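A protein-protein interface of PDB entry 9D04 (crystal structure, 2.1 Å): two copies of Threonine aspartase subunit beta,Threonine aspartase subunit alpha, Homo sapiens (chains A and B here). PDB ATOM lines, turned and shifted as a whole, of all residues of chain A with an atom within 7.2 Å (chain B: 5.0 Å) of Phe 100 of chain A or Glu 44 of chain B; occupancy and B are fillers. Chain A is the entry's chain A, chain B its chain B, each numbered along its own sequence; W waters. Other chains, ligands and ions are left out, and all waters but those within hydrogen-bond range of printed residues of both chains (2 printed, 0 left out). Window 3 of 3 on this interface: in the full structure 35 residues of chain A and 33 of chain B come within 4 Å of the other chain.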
ATOM      1  N   GLU A  63     -23.732   7.854 -29.704  1.00  0.00           N
ATOM      2  CA  GLU A  63     -22.654   6.876 -29.619  1.00  0.00           C
ATOM      3  C   GLU A  63     -22.106   6.731 -28.206  1.00  0.00           C
ATOM      4  O   GLU A  63     -21.685   5.632 -27.833  1.00  0.00           O
ATOM      5  CB  GLU A  63     -21.525   7.260 -30.566  1.00  0.00           C
ATOM      6  CG  GLU A  63     -21.885   7.120 -32.028  1.00  0.00           C
ATOM      7  CD  GLU A  63     -21.992   5.676 -32.465  1.00  0.00           C
ATOM      8  OE1 GLU A  63     -23.095   5.241 -32.875  1.00  0.00           O
ATOM      9  OE2 GLU A  63     -20.963   4.976 -32.387  1.00  0.00           O
ATOM     10  N   HIS A  64     -22.168   7.796 -27.396  1.00  0.00           N
ATOM     11  CA  HIS A  64     -21.717   7.718 -26.010  1.00  0.00           C
ATOM     12  C   HIS A  64     -22.598   6.789 -25.184  1.00  0.00           C
ATOM     13  O   HIS A  64     -22.112   6.076 -24.298  1.00  0.00           O
ATOM     14  CB  HIS A  64     -21.736   9.112 -25.368  1.00  0.00           C
ATOM     15  CG  HIS A  64     -20.936  10.152 -26.094  1.00  0.00           C
ATOM     16  ND1 HIS A  64     -21.042  11.495 -25.807  1.00  0.00           N
ATOM     17  CD2 HIS A  64     -19.996  10.050 -27.068  1.00  0.00           C
ATOM     18  CE1 HIS A  64     -20.220  12.179 -26.583  1.00  0.00           C
ATOM     19  NE2 HIS A  64     -19.570  11.325 -27.354  1.00  0.00           N
ATOM     20  N   VAL A  66     -24.383   4.204 -26.400  1.00  0.00           N
ATOM     21  CA  VAL A  66     -24.133   2.825 -26.841  1.00  0.00           C
ATOM     22  C   VAL A  66     -22.903   2.258 -26.150  1.00  0.00           C
ATOM     23  O   VAL A  66     -22.966   1.198 -25.517  1.00  0.00           O
ATOM     24  CB  VAL A  66     -23.971   2.752 -28.370  1.00  0.00           C
ATOM     25  CG1 VAL A  66     -23.654   1.310 -28.797  1.00  0.00           C
ATOM     26  CG2 VAL A  66     -25.222   3.275 -29.079  1.00  0.00           C
ATOM     27  N   ARG A  67     -21.756   2.940 -26.296  1.00  0.00           N
ATOM     28  CA  ARG A  67     -20.484   2.368 -25.859  1.00  0.00           C
ATOM     29  C   ARG A  67     -20.496   2.007 -24.380  1.00  0.00           C
ATOM     30  O   ARG A  67     -19.798   1.075 -23.965  1.00  0.00           O
ATOM     31  CB  ARG A  67     -19.316   3.308 -26.164  1.00  0.00           C
ATOM     32  CG  ARG A  67     -19.184   3.716 -27.632  1.00  0.00           C
ATOM     33  CD  ARG A  67     -19.369   2.548 -28.578  1.00  0.00           C
ATOM     34  NE  ARG A  67     -19.044   2.907 -29.958  1.00  0.00           N
ATOM     35  CZ  ARG A  67     -17.810   2.933 -30.453  1.00  0.00           C
ATOM     36  NH1 ARG A  67     -17.609   3.281 -31.714  1.00  0.00           N
ATOM     37  NH2 ARG A  67     -16.778   2.593 -29.694  1.00  0.00           N
ATOM     38  N   THR A  68     -21.301   2.708 -23.583  1.00  0.00           N
ATOM     39  CA  THR A  68     -21.354   2.501 -22.145  1.00  0.00           C
ATOM     40  C   THR A  68     -22.555   1.661 -21.713  1.00  0.00           C
ATOM     41  O   THR A  68     -22.679   1.351 -20.524  1.00  0.00           O
ATOM     42  CB  THR A  68     -21.395   3.865 -21.441  1.00  0.00           C
ATOM     43  OG1 THR A  68     -22.536   4.600 -21.902  1.00  0.00           O
ATOM     44  CG2 THR A  68     -20.125   4.668 -21.755  1.00  0.00           C
ATOM     45  N   LYS A  94     -19.214   5.703 -14.857  1.00  0.00           N
ATOM     46  CA  LYS A  94     -19.539   4.795 -15.950  1.00  0.00           C
ATOM     47  C   LYS A  94     -19.835   5.536 -17.253  1.00  0.00           C
ATOM     48  O   LYS A  94     -19.864   4.913 -18.320  1.00  0.00           O
ATOM     49  CB  LYS A  94     -20.738   3.913 -15.561  1.00  0.00           C
ATOM     50  CG  LYS A  94     -20.499   2.978 -14.358  1.00  0.00           C
ATOM     51  CD  LYS A  94     -19.291   2.086 -14.557  1.00  0.00           C
ATOM     52  CE  LYS A  94     -19.440   0.791 -13.761  1.00  0.00           C
ATOM     53  NZ  LYS A  94     -18.440  -0.254 -14.159  1.00  0.00           N
ATOM     54  N   PHE A  95     -20.187   6.813 -17.175  1.00  0.00           N
ATOM     55  CA  PHE A  95     -20.491   7.596 -18.368  1.00  0.00           C
ATOM     56  C   PHE A  95     -19.357   8.589 -18.650  1.00  0.00           C
ATOM     57  O   PHE A  95     -18.497   8.316 -19.491  1.00  0.00           O
ATOM     58  CB  PHE A  95     -21.859   8.267 -18.184  1.00  0.00           C
ATOM     59  CG  PHE A  95     -22.448   8.849 -19.444  1.00  0.00           C
ATOM     60  CD1 PHE A  95     -22.537   8.093 -20.611  1.00  0.00           C
ATOM     61  CD2 PHE A  95     -22.947  10.150 -19.441  1.00  0.00           C
ATOM     62  CE1 PHE A  95     -23.100   8.626 -21.761  1.00  0.00           C
ATOM     63  CE2 PHE A  95     -23.504  10.700 -20.579  1.00  0.00           C
ATOM     64  CZ  PHE A  95     -23.588   9.935 -21.751  1.00  0.00           C
ATOM     65  N   SER A  97     -16.532   9.302 -17.202  1.00  0.00           N
ATOM     66  CA  SER A  97     -15.160   8.819 -17.065  1.00  0.00           C
ATOM     67  C   SER A  97     -14.990   7.407 -17.599  1.00  0.00           C
ATOM     68  O   SER A  97     -14.025   6.728 -17.252  1.00  0.00           O
ATOM     69  CB  SER A  97     -14.694   8.887 -15.605  1.00  0.00           C
ATOM     70  OG  SER A  97     -14.643  10.226 -15.164  1.00  0.00           O
ATOM     71  N   SER A  98     -15.905   6.941 -18.436  1.00  0.00           N
ATOM     72  CA  SER A  98     -15.764   5.593 -18.957  1.00  0.00           C
ATOM     73  C   SER A  98     -14.506   5.506 -19.812  1.00  0.00           C
ATOM     74  O   SER A  98     -14.238   6.403 -20.619  1.00  0.00           O
ATOM     75  CB  SER A  98     -16.978   5.197 -19.803  1.00  0.00           C
ATOM     76  OG  SER A  98     -16.750   3.920 -20.387  1.00  0.00           O
ATOM     77  N   PRO A  99     -13.726   4.432 -19.686  1.00  0.00           N
ATOM     78  CA  PRO A  99     -12.631   4.225 -20.639  1.00  0.00           C
ATOM     79  C   PRO A  99     -13.141   4.042 -22.062  1.00  0.00           C
ATOM     80  O   PRO A  99     -12.370   4.232 -23.017  1.00  0.00           O
ATOM     81  CB  PRO A  99     -11.927   2.969 -20.106  1.00  0.00           C
ATOM     82  CG  PRO A  99     -12.997   2.235 -19.358  1.00  0.00           C
ATOM     83  CD  PRO A  99     -13.885   3.299 -18.757  1.00  0.00           C
ATOM     84  N   PHE A 100     -14.420   3.684 -22.229  1.00  0.00           N
ATOM     85  CA  PHE A 100     -14.992   3.482 -23.553  1.00  0.00           C
ATOM     86  C   PHE A 100     -15.177   4.785 -24.315  1.00  0.00           C
ATOM     87  O   PHE A 100     -15.413   4.743 -25.525  1.00  0.00           O
ATOM     88  CB  PHE A 100     -16.323   2.730 -23.429  1.00  0.00           C
ATOM     89  CG  PHE A 100     -16.143   1.315 -22.995  1.00  0.00           C
ATOM     90  CD1 PHE A 100     -16.038   1.005 -21.643  1.00  0.00           C
ATOM     91  CD2 PHE A 100     -15.974   0.308 -23.928  1.00  0.00           C
ATOM     92  CE1 PHE A 100     -15.823  -0.303 -21.225  1.00  0.00           C
ATOM     93  CE2 PHE A 100     -15.756  -1.000 -23.523  1.00  0.00           C
ATOM     94  CZ  PHE A 100     -15.677  -1.307 -22.162  1.00  0.00           C
ATOM     95  N   LEU A 101     -15.035   5.934 -23.649  1.00  0.00           N
ATOM     96  CA  LEU A 101     -15.168   7.234 -24.295  1.00  0.00           C
ATOM     97  C   LEU A 101     -13.985   8.142 -23.981  1.00  0.00           C
ATOM     98  O   LEU A 101     -14.127   9.369 -24.019  1.00  0.00           O
ATOM     99  CB  LEU A 101     -16.469   7.918 -23.868  1.00  0.00           C
ATOM    100  CG  LEU A 101     -17.744   7.092 -24.013  1.00  0.00           C
ATOM    101  CD1 LEU A 101     -18.868   7.694 -23.197  1.00  0.00           C
ATOM    102  CD2 LEU A 101     -18.081   7.046 -25.481  1.00  0.00           C
ATOM    103  N   ALA A 102     -12.826   7.566 -23.661  1.00  0.00           N
ATOM    104  CA  ALA A 102     -11.693   8.363 -23.203  1.00  0.00           C
ATOM    105  C   ALA A 102     -11.126   9.263 -24.297  1.00  0.00           C
ATOM    106  O   ALA A 102     -10.489  10.273 -23.976  1.00  0.00           O
ATOM    107  CB  ALA A 102     -10.598   7.449 -22.652  1.00  0.00           C
ATOM    108  N   SER A 103     -11.350   8.931 -25.574  1.00  0.00           N
ATOM    109  CA  SER A 103     -10.881   9.769 -26.675  1.00  0.00           C
ATOM    110  C   SER A 103     -11.725  11.022 -26.881  1.00  0.00           C
ATOM    111  O   SER A 103     -11.289  11.930 -27.595  1.00  0.00           O
ATOM    112  CB  SER A 103     -10.860   8.971 -27.984  1.00  0.00           C
ATOM    113  OG  SER A 103     -10.002   7.849 -27.899  1.00  0.00           O
ATOM    114  N   GLU A 104     -12.912  11.098 -26.290  1.00  0.00           N
ATOM    115  CA  GLU A 104     -13.852  12.165 -26.594  1.00  0.00           C
ATOM    116  C   GLU A 104     -13.638  13.374 -25.693  1.00  0.00           C
ATOM    117  O   GLU A 104     -13.356  13.235 -24.499  1.00  0.00           O
ATOM    118  CB  GLU A 104     -15.294  11.674 -26.451  1.00  0.00           C
ATOM    119  CG  GLU A 104     -15.614  10.432 -27.282  1.00  0.00           C
ATOM    120  CD  GLU A 104     -15.082  10.531 -28.697  1.00  0.00           C
ATOM    121  OE1 GLU A 104     -15.320  11.570 -29.354  1.00  0.00           O
ATOM    122  OE2 GLU A 104     -14.406   9.577 -29.145  1.00  0.00           O
ATOM    123  N   VAL B  14      -6.061  -7.722 -27.511  1.00  0.00           N
ATOM    124  CA  VAL B  14      -7.026  -8.731 -27.921  1.00  0.00           C
ATOM    125  C   VAL B  14      -8.038  -8.124 -28.891  1.00  0.00           C
ATOM    126  O   VAL B  14      -8.242  -6.901 -28.965  1.00  0.00           O
ATOM    127  CB  VAL B  14      -7.760  -9.380 -26.728  1.00  0.00           C
ATOM    128  CG1 VAL B  14      -6.750 -10.098 -25.799  1.00  0.00           C
ATOM    129  CG2 VAL B  14      -8.607  -8.336 -25.987  1.00  0.00           C
ATOM    130  N   TYR B  37     -23.925  -4.686 -30.185  1.00  0.00           N
ATOM    131  CA  TYR B  37     -22.883  -4.349 -29.215  1.00  0.00           C
ATOM    132  C   TYR B  37     -23.104  -5.065 -27.889  1.00  0.00           C
ATOM    133  O   TYR B  37     -24.208  -5.050 -27.336  1.00  0.00           O
ATOM    134  CB  TYR B  37     -22.895  -2.835 -28.988  1.00  0.00           C
ATOM    135  CG  TYR B  37     -21.757  -2.282 -28.164  1.00  0.00           C
ATOM    136  CD1 TYR B  37     -20.458  -2.245 -28.669  1.00  0.00           C
ATOM    137  CD2 TYR B  37     -21.993  -1.752 -26.889  1.00  0.00           C
ATOM    138  CE1 TYR B  37     -19.409  -1.707 -27.905  1.00  0.00           C
ATOM    139  CE2 TYR B  37     -20.956  -1.214 -26.125  1.00  0.00           C
ATOM    140  CZ  TYR B  37     -19.667  -1.197 -26.637  1.00  0.00           C
ATOM    141  OH  TYR B  37     -18.644  -0.651 -25.879  1.00  0.00           O
ATOM    142  N   TRP B  42     -17.068  -9.383 -27.797  1.00  0.00           N
ATOM    143  CA  TRP B  42     -16.549  -8.397 -26.852  1.00  0.00           C
ATOM    144  C   TRP B  42     -15.034  -8.532 -26.769  1.00  0.00           C
ATOM    145  O   TRP B  42     -14.505  -9.646 -26.807  1.00  0.00           O
ATOM    146  CB  TRP B  42     -17.153  -8.582 -25.450  1.00  0.00           C
ATOM    147  CG  TRP B  42     -16.940  -7.397 -24.525  1.00  0.00           C
ATOM    148  CD1 TRP B  42     -15.975  -7.263 -23.531  1.00  0.00           C
ATOM    149  CD2 TRP B  42     -17.690  -6.179 -24.516  1.00  0.00           C
ATOM    150  NE1 TRP B  42     -16.110  -6.045 -22.910  1.00  0.00           N
ATOM    151  CE2 TRP B  42     -17.145  -5.354 -23.497  1.00  0.00           C
ATOM    152  CE3 TRP B  42     -18.766  -5.695 -25.280  1.00  0.00           C
ATOM    153  CZ2 TRP B  42     -17.653  -4.086 -23.208  1.00  0.00           C
ATOM    154  CZ3 TRP B  42     -19.271  -4.423 -24.995  1.00  0.00           C
ATOM    155  CH2 TRP B  42     -18.711  -3.635 -23.974  1.00  0.00           C
ATOM    156  N   ALA B  43     -14.338  -7.400 -26.702  1.00  0.00           N
ATOM    157  CA  ALA B  43     -12.898  -7.434 -26.494  1.00  0.00           C
ATOM    158  C   ALA B  43     -12.490  -6.227 -25.658  1.00  0.00           C
ATOM    159  O   ALA B  43     -12.901  -5.098 -25.940  1.00  0.00           O
ATOM    160  CB  ALA B  43     -12.123  -7.500 -27.822  1.00  0.00           C
ATOM    161  N   GLU B  44     -11.695  -6.472 -24.613  1.00  0.00           N
ATOM    162  CA  GLU B  44     -11.358  -5.418 -23.662  1.00  0.00           C
ATOM    163  C   GLU B  44      -9.990  -5.717 -23.066  1.00  0.00           C
ATOM    164  O   GLU B  44      -9.827  -6.725 -22.368  1.00  0.00           O
ATOM    165  CB  GLU B  44     -12.445  -5.326 -22.568  1.00  0.00           C
ATOM    166  CG  GLU B  44     -12.207  -4.291 -21.469  1.00  0.00           C
ATOM    167  CD  GLU B  44     -13.419  -4.136 -20.538  1.00  0.00           C
ATOM    168  OE1 GLU B  44     -14.444  -4.832 -20.744  1.00  0.00           O
ATOM    169  OE2 GLU B  44     -13.342  -3.335 -19.582  1.00  0.00           O
ATOM    170  N   ASN B  45      -9.013  -4.849 -23.333  1.00  0.00           N
ATOM    171  CA  ASN B  45      -7.686  -5.043 -22.759  1.00  0.00           C
ATOM    172  C   ASN B  45      -7.751  -4.894 -21.243  1.00  0.00           C
ATOM    173  O   ASN B  45      -8.714  -4.357 -20.680  1.00  0.00           O
ATOM    174  CB  ASN B  45      -6.666  -4.038 -23.322  1.00  0.00           C
ATOM    175  CG  ASN B  45      -6.062  -4.493 -24.646  1.00  0.00           C
ATOM    176  OD1 ASN B  45      -6.552  -5.432 -25.265  1.00  0.00           O
ATOM    177  ND2 ASN B  45      -4.992  -3.839 -25.070  1.00  0.00           N
ATOM    178  N   THR B  46      -6.714  -5.392 -20.581  1.00  0.00           N
ATOM    179  CA  THR B  46      -6.611  -5.219 -19.142  1.00  0.00           C
ATOM    180  C   THR B  46      -6.667  -3.728 -18.813  1.00  0.00           C
ATOM    181  O   THR B  46      -6.118  -2.890 -19.538  1.00  0.00           O
ATOM    182  CB  THR B  46      -5.311  -5.862 -18.623  1.00  0.00           C
ATOM    183  OG1 THR B  46      -5.152  -5.611 -17.217  1.00  0.00           O
ATOM    184  CG2 THR B  46      -4.110  -5.304 -19.359  1.00  0.00           C
ATOM    185  N   ASN B  50     -10.215  -4.601 -14.361  1.00  0.00           N
ATOM    186  CA  ASN B  50     -10.175  -5.611 -15.412  1.00  0.00           C
ATOM    187  C   ASN B  50      -8.770  -6.190 -15.524  1.00  0.00           C
ATOM    188  O   ASN B  50      -8.005  -5.764 -16.394  1.00  0.00           O
ATOM    189  CB  ASN B  50     -10.601  -4.992 -16.748  1.00  0.00           C
ATOM    190  CG  ASN B  50     -11.538  -5.885 -17.540  1.00  0.00           C
ATOM    191  OD1 ASN B  50     -12.689  -6.090 -17.149  1.00  0.00           O
ATOM    192  ND2 ASN B  50     -11.061  -6.395 -18.678  1.00  0.00           N
ATOM    193  N   TYR B  52      -7.556  -8.964 -16.648  1.00  0.00           N
ATOM    194  CA  TYR B  52      -7.252  -9.771 -17.817  1.00  0.00           C
ATOM    195  C   TYR B  52      -7.704  -9.053 -19.076  1.00  0.00           C
ATOM    196  O   TYR B  52      -8.793  -8.473 -19.113  1.00  0.00           O
ATOM    197  CB  TYR B  52      -7.930 -11.143 -17.733  1.00  0.00           C
ATOM    198  CG  TYR B  52      -7.401 -12.036 -16.632  1.00  0.00           C
ATOM    199  CD1 TYR B  52      -6.330 -12.884 -16.867  1.00  0.00           C
ATOM    200  CD2 TYR B  52      -7.978 -12.043 -15.366  1.00  0.00           C
ATOM    201  CE1 TYR B  52      -5.837 -13.716 -15.870  1.00  0.00           C
ATOM    202  CE2 TYR B  52      -7.484 -12.871 -14.349  1.00  0.00           C
ATOM    203  CZ  TYR B  52      -6.413 -13.705 -14.612  1.00  0.00           C
ATOM    204  OH  TYR B  52      -5.908 -14.542 -13.630  1.00  0.00           O
ATOM    205  N   SER B  53      -6.890  -9.139 -20.125  1.00  0.00           N
ATOM    206  CA  SER B  53      -7.355  -8.770 -21.455  1.00  0.00           C
ATOM    207  C   SER B  53      -8.224  -9.917 -21.946  1.00  0.00           C
ATOM    208  O   SER B  53      -7.764 -11.060 -21.989  1.00  0.00           O
ATOM    209  CB  SER B  53      -6.181  -8.527 -22.400  1.00  0.00           C
ATOM    210  OG  SER B  53      -5.342  -7.472 -21.958  1.00  0.00           O
ATOM    211  N   THR B  54      -9.481  -9.633 -22.298  1.00  0.00           N
ATOM    212  CA  THR B  54     -10.449 -10.684 -22.562  1.00  0.00           C
ATOM    213  C   THR B  54     -11.136 -10.447 -23.901  1.00  0.00           C
ATOM    214  O   THR B  54     -11.393  -9.305 -24.292  1.00  0.00           O
ATOM    215  CB  THR B  54     -11.471 -10.759 -21.416  1.00  0.00           C
ATOM    216  OG1 THR B  54     -10.778 -10.944 -20.174  1.00  0.00           O
ATOM    217  CG2 THR B  54     -12.455 -11.903 -21.617  1.00  0.00           C
ATOM    218  N   SER B  75     -17.184 -11.848 -20.628  1.00  0.00           N
ATOM    219  CA  SER B  75     -15.955 -11.096 -20.415  1.00  0.00           C
ATOM    220  C   SER B  75     -15.854 -10.608 -18.981  1.00  0.00           C
ATOM    221  O   SER B  75     -14.791 -10.713 -18.356  1.00  0.00           O
ATOM    222  CB  SER B  75     -15.887  -9.916 -21.387  1.00  0.00           C
ATOM    223  OG  SER B  75     -14.704  -9.171 -21.154  1.00  0.00           O
ATOM    224  N   HIS B  76     -16.959 -10.105 -18.427  1.00  0.00           N
ATOM    225  CA  HIS B  76     -16.922  -9.657 -17.046  1.00  0.00           C
ATOM    226  C   HIS B  76     -16.737 -10.830 -16.093  1.00  0.00           C
ATOM    227  O   HIS B  76     -15.983 -10.722 -15.123  1.00  0.00           O
ATOM    228  CB  HIS B  76     -18.186  -8.869 -16.701  1.00  0.00           C
ATOM    229  CG  HIS B  76     -18.243  -7.512 -17.342  1.00  0.00           C
ATOM    230  ND1 HIS B  76     -19.229  -6.591 -17.055  1.00  0.00           N
ATOM    231  CD2 HIS B  76     -17.442  -6.927 -18.264  1.00  0.00           C
ATOM    232  CE1 HIS B  76     -19.025  -5.494 -17.762  1.00  0.00           C
ATOM    233  NE2 HIS B  76     -17.946  -5.671 -18.502  1.00  0.00           N
ATOM    234  N   MET B 268     -14.813  -6.105 -32.342  1.00  0.00           N
ATOM    235  CA  MET B 268     -14.446  -5.184 -31.274  1.00  0.00           C
ATOM    236  C   MET B 268     -12.940  -5.258 -31.055  1.00  0.00           C
ATOM    237  O   MET B 268     -12.340  -6.333 -31.182  1.00  0.00           O
ATOM    238  CB  MET B 268     -15.206  -5.505 -29.983  1.00  0.00           C
ATOM    239  CG  MET B 268     -15.027  -4.470 -28.857  1.00  0.00           C
ATOM    240  SD  MET B 268     -16.306  -4.692 -27.646  1.00  0.00           S
ATOM    241  CE  MET B 268     -15.928  -3.428 -26.400  1.00  0.00           C
ATOM    242  N   GLY B 270      -9.853  -4.689 -28.436  1.00  0.00           N
ATOM    243  CA  GLY B 270      -9.646  -4.597 -26.997  1.00  0.00           C
ATOM    244  C   GLY B 270      -8.822  -3.395 -26.558  1.00  0.00           C
ATOM    245  O   GLY B 270      -8.978  -2.909 -25.432  1.00  0.00           O
ATOM    246  N   LEU B 273     -11.045  -0.181 -27.577  1.00  0.00           N
ATOM    247  CA  LEU B 273     -12.443  -0.450 -27.246  1.00  0.00           C
ATOM    248  C   LEU B 273     -13.392  -0.053 -28.376  1.00  0.00           C
ATOM    249  O   LEU B 273     -14.614  -0.023 -28.180  1.00  0.00           O
ATOM    250  CB  LEU B 273     -12.858   0.214 -25.921  1.00  0.00           C
ATOM    251  CG  LEU B 273     -12.001  -0.198 -24.707  1.00  0.00           C
ATOM    252  CD1 LEU B 273     -12.343   0.597 -23.440  1.00  0.00           C
ATOM    253  CD2 LEU B 273     -12.079  -1.718 -24.421  1.00  0.00           C
HETATM  254  O   HOH W   1     -16.990   0.694 -27.428  1.00  0.00           O
HETATM  255  O   HOH W   2     -15.138   3.185 -27.491  1.00  0.00           O
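The backbone carbonyl oxygen (O) of Arg 67 of chain A sits at hydrogen-bond distance from the side-chain hydroxyl (OH) of Tyr 37 of chain B.
The backbone carbonyl oxygen (O) of Thr 54 of chain B lies within hydrogen-bond range of the backbone NH (N) of Glu 44 of chain B (2.9 Å). The backbone NH of Ala 43 of chain B sits at hydrogen-bond distance from the side-chain sulfur of Met 268 of chain B. The side-chain carboxylate of Glu 44 of chain B is in hydrogen-bond range of the indole nitrogen of Trp 42 of chain B (3.0 Å). The backbone NH (N) of Phe 100 of chain A lies within hydrogen-bond range of the side-chain hydroxyl (OG) of Ser 98 of chain A (3.0 Å). The side-chain carboxylate (OE2) of Glu 63 of chain A lies within salt-bridge range of the guanidinium group (NE) of Arg 67 of chain A.
CE2 of Tyr 37 of chain B touches O of Val 66 of chain A (3.2 Å). Arg 67 of chain A touches Leu 273 of chain B (NH2 to O, 3.7 Å). Leu 273 of chain B touches Pro 99 of chain A. CD2 of Phe 100 of chain A touches OH of Tyr 37 of chain B, 3.4 Å away. Trp 42 of chain B touches Phe 100 of chain A (CZ2 to CZ, 3.6 Å). Phe 100 of chain A touches Glu 44 of chain B. Phe 100 of chain A touches Met 268 of chain B (CE2 to CE, 3.8 Å). Phe 100 of chain A touches Leu 273 of chain B (CD2 to CD1, 3.7 Å).
Of the printed residues of chain B, Arg 67 of chain A touches Tyr 37 (2.8 Å) and Leu 273 (3.7 Å). Printed residues of chain B within 4 Å of Pro 99 of chain A: Leu 273 (3.7 Å). Phe 100 of chain A touches just these residues of chain B: Tyr 37 (3.4 Å), Trp 42 (3.6 Å), Glu 44 (3.97 Å), Met 268 (3.8 Å) and Leu 273 (3.7 Å). Of the printed residues of chain A, Trp 42 of chain B touches Phe 100. Glu 44 of chain B touches just one residue of chain A: Phe 100 (3.97 Å). Tyr 52 of chain B touches none of the printed residues of chain A. Of the printed residues of chain A, Met 268 of chain B touches Phe 100 (3.8 Å). Printed residues of chain A within 4 Å of Leu 273 of chain B: Arg 67 (3.7 Å), Pro 99 (3.7 Å) and Phe 100 (3.7 Å). The nearest residue of chain A that does not touch Glu 44 of chain B is Pro 99 of chain A (5.6 Å).
Of the 16 printed residues of chain B, 5 touch a printed residue of chain A. Of the 15 printed residues of chain A, 4 touch a printed residue of chain B. Among the printed residues, 9 pairs touch across the chains. Among the printed residues, no Asp or Glu carboxylate lies within 4 Å of a Lys or Arg side-chain nitrogen of the other chain.
No position is printed for both chains.
Water W2 lies within hydrogen-bond range of the backbone carbonyl oxygen (O) of Phe 100 of chain A (2.5 Å), the guanidinium group (NH2) of Arg 67 of chain A (2.8 Å) and the backbone carbonyl oxygen (O) of Leu 273 of chain B (3.3 Å). Water W1 lies within hydrogen-bond range of O of Leu 273 of chain B (2.6 Å), OH of Tyr 37 of chain B (2.6 Å) and NH2 of Arg 67 of chain A (3.0 Å).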
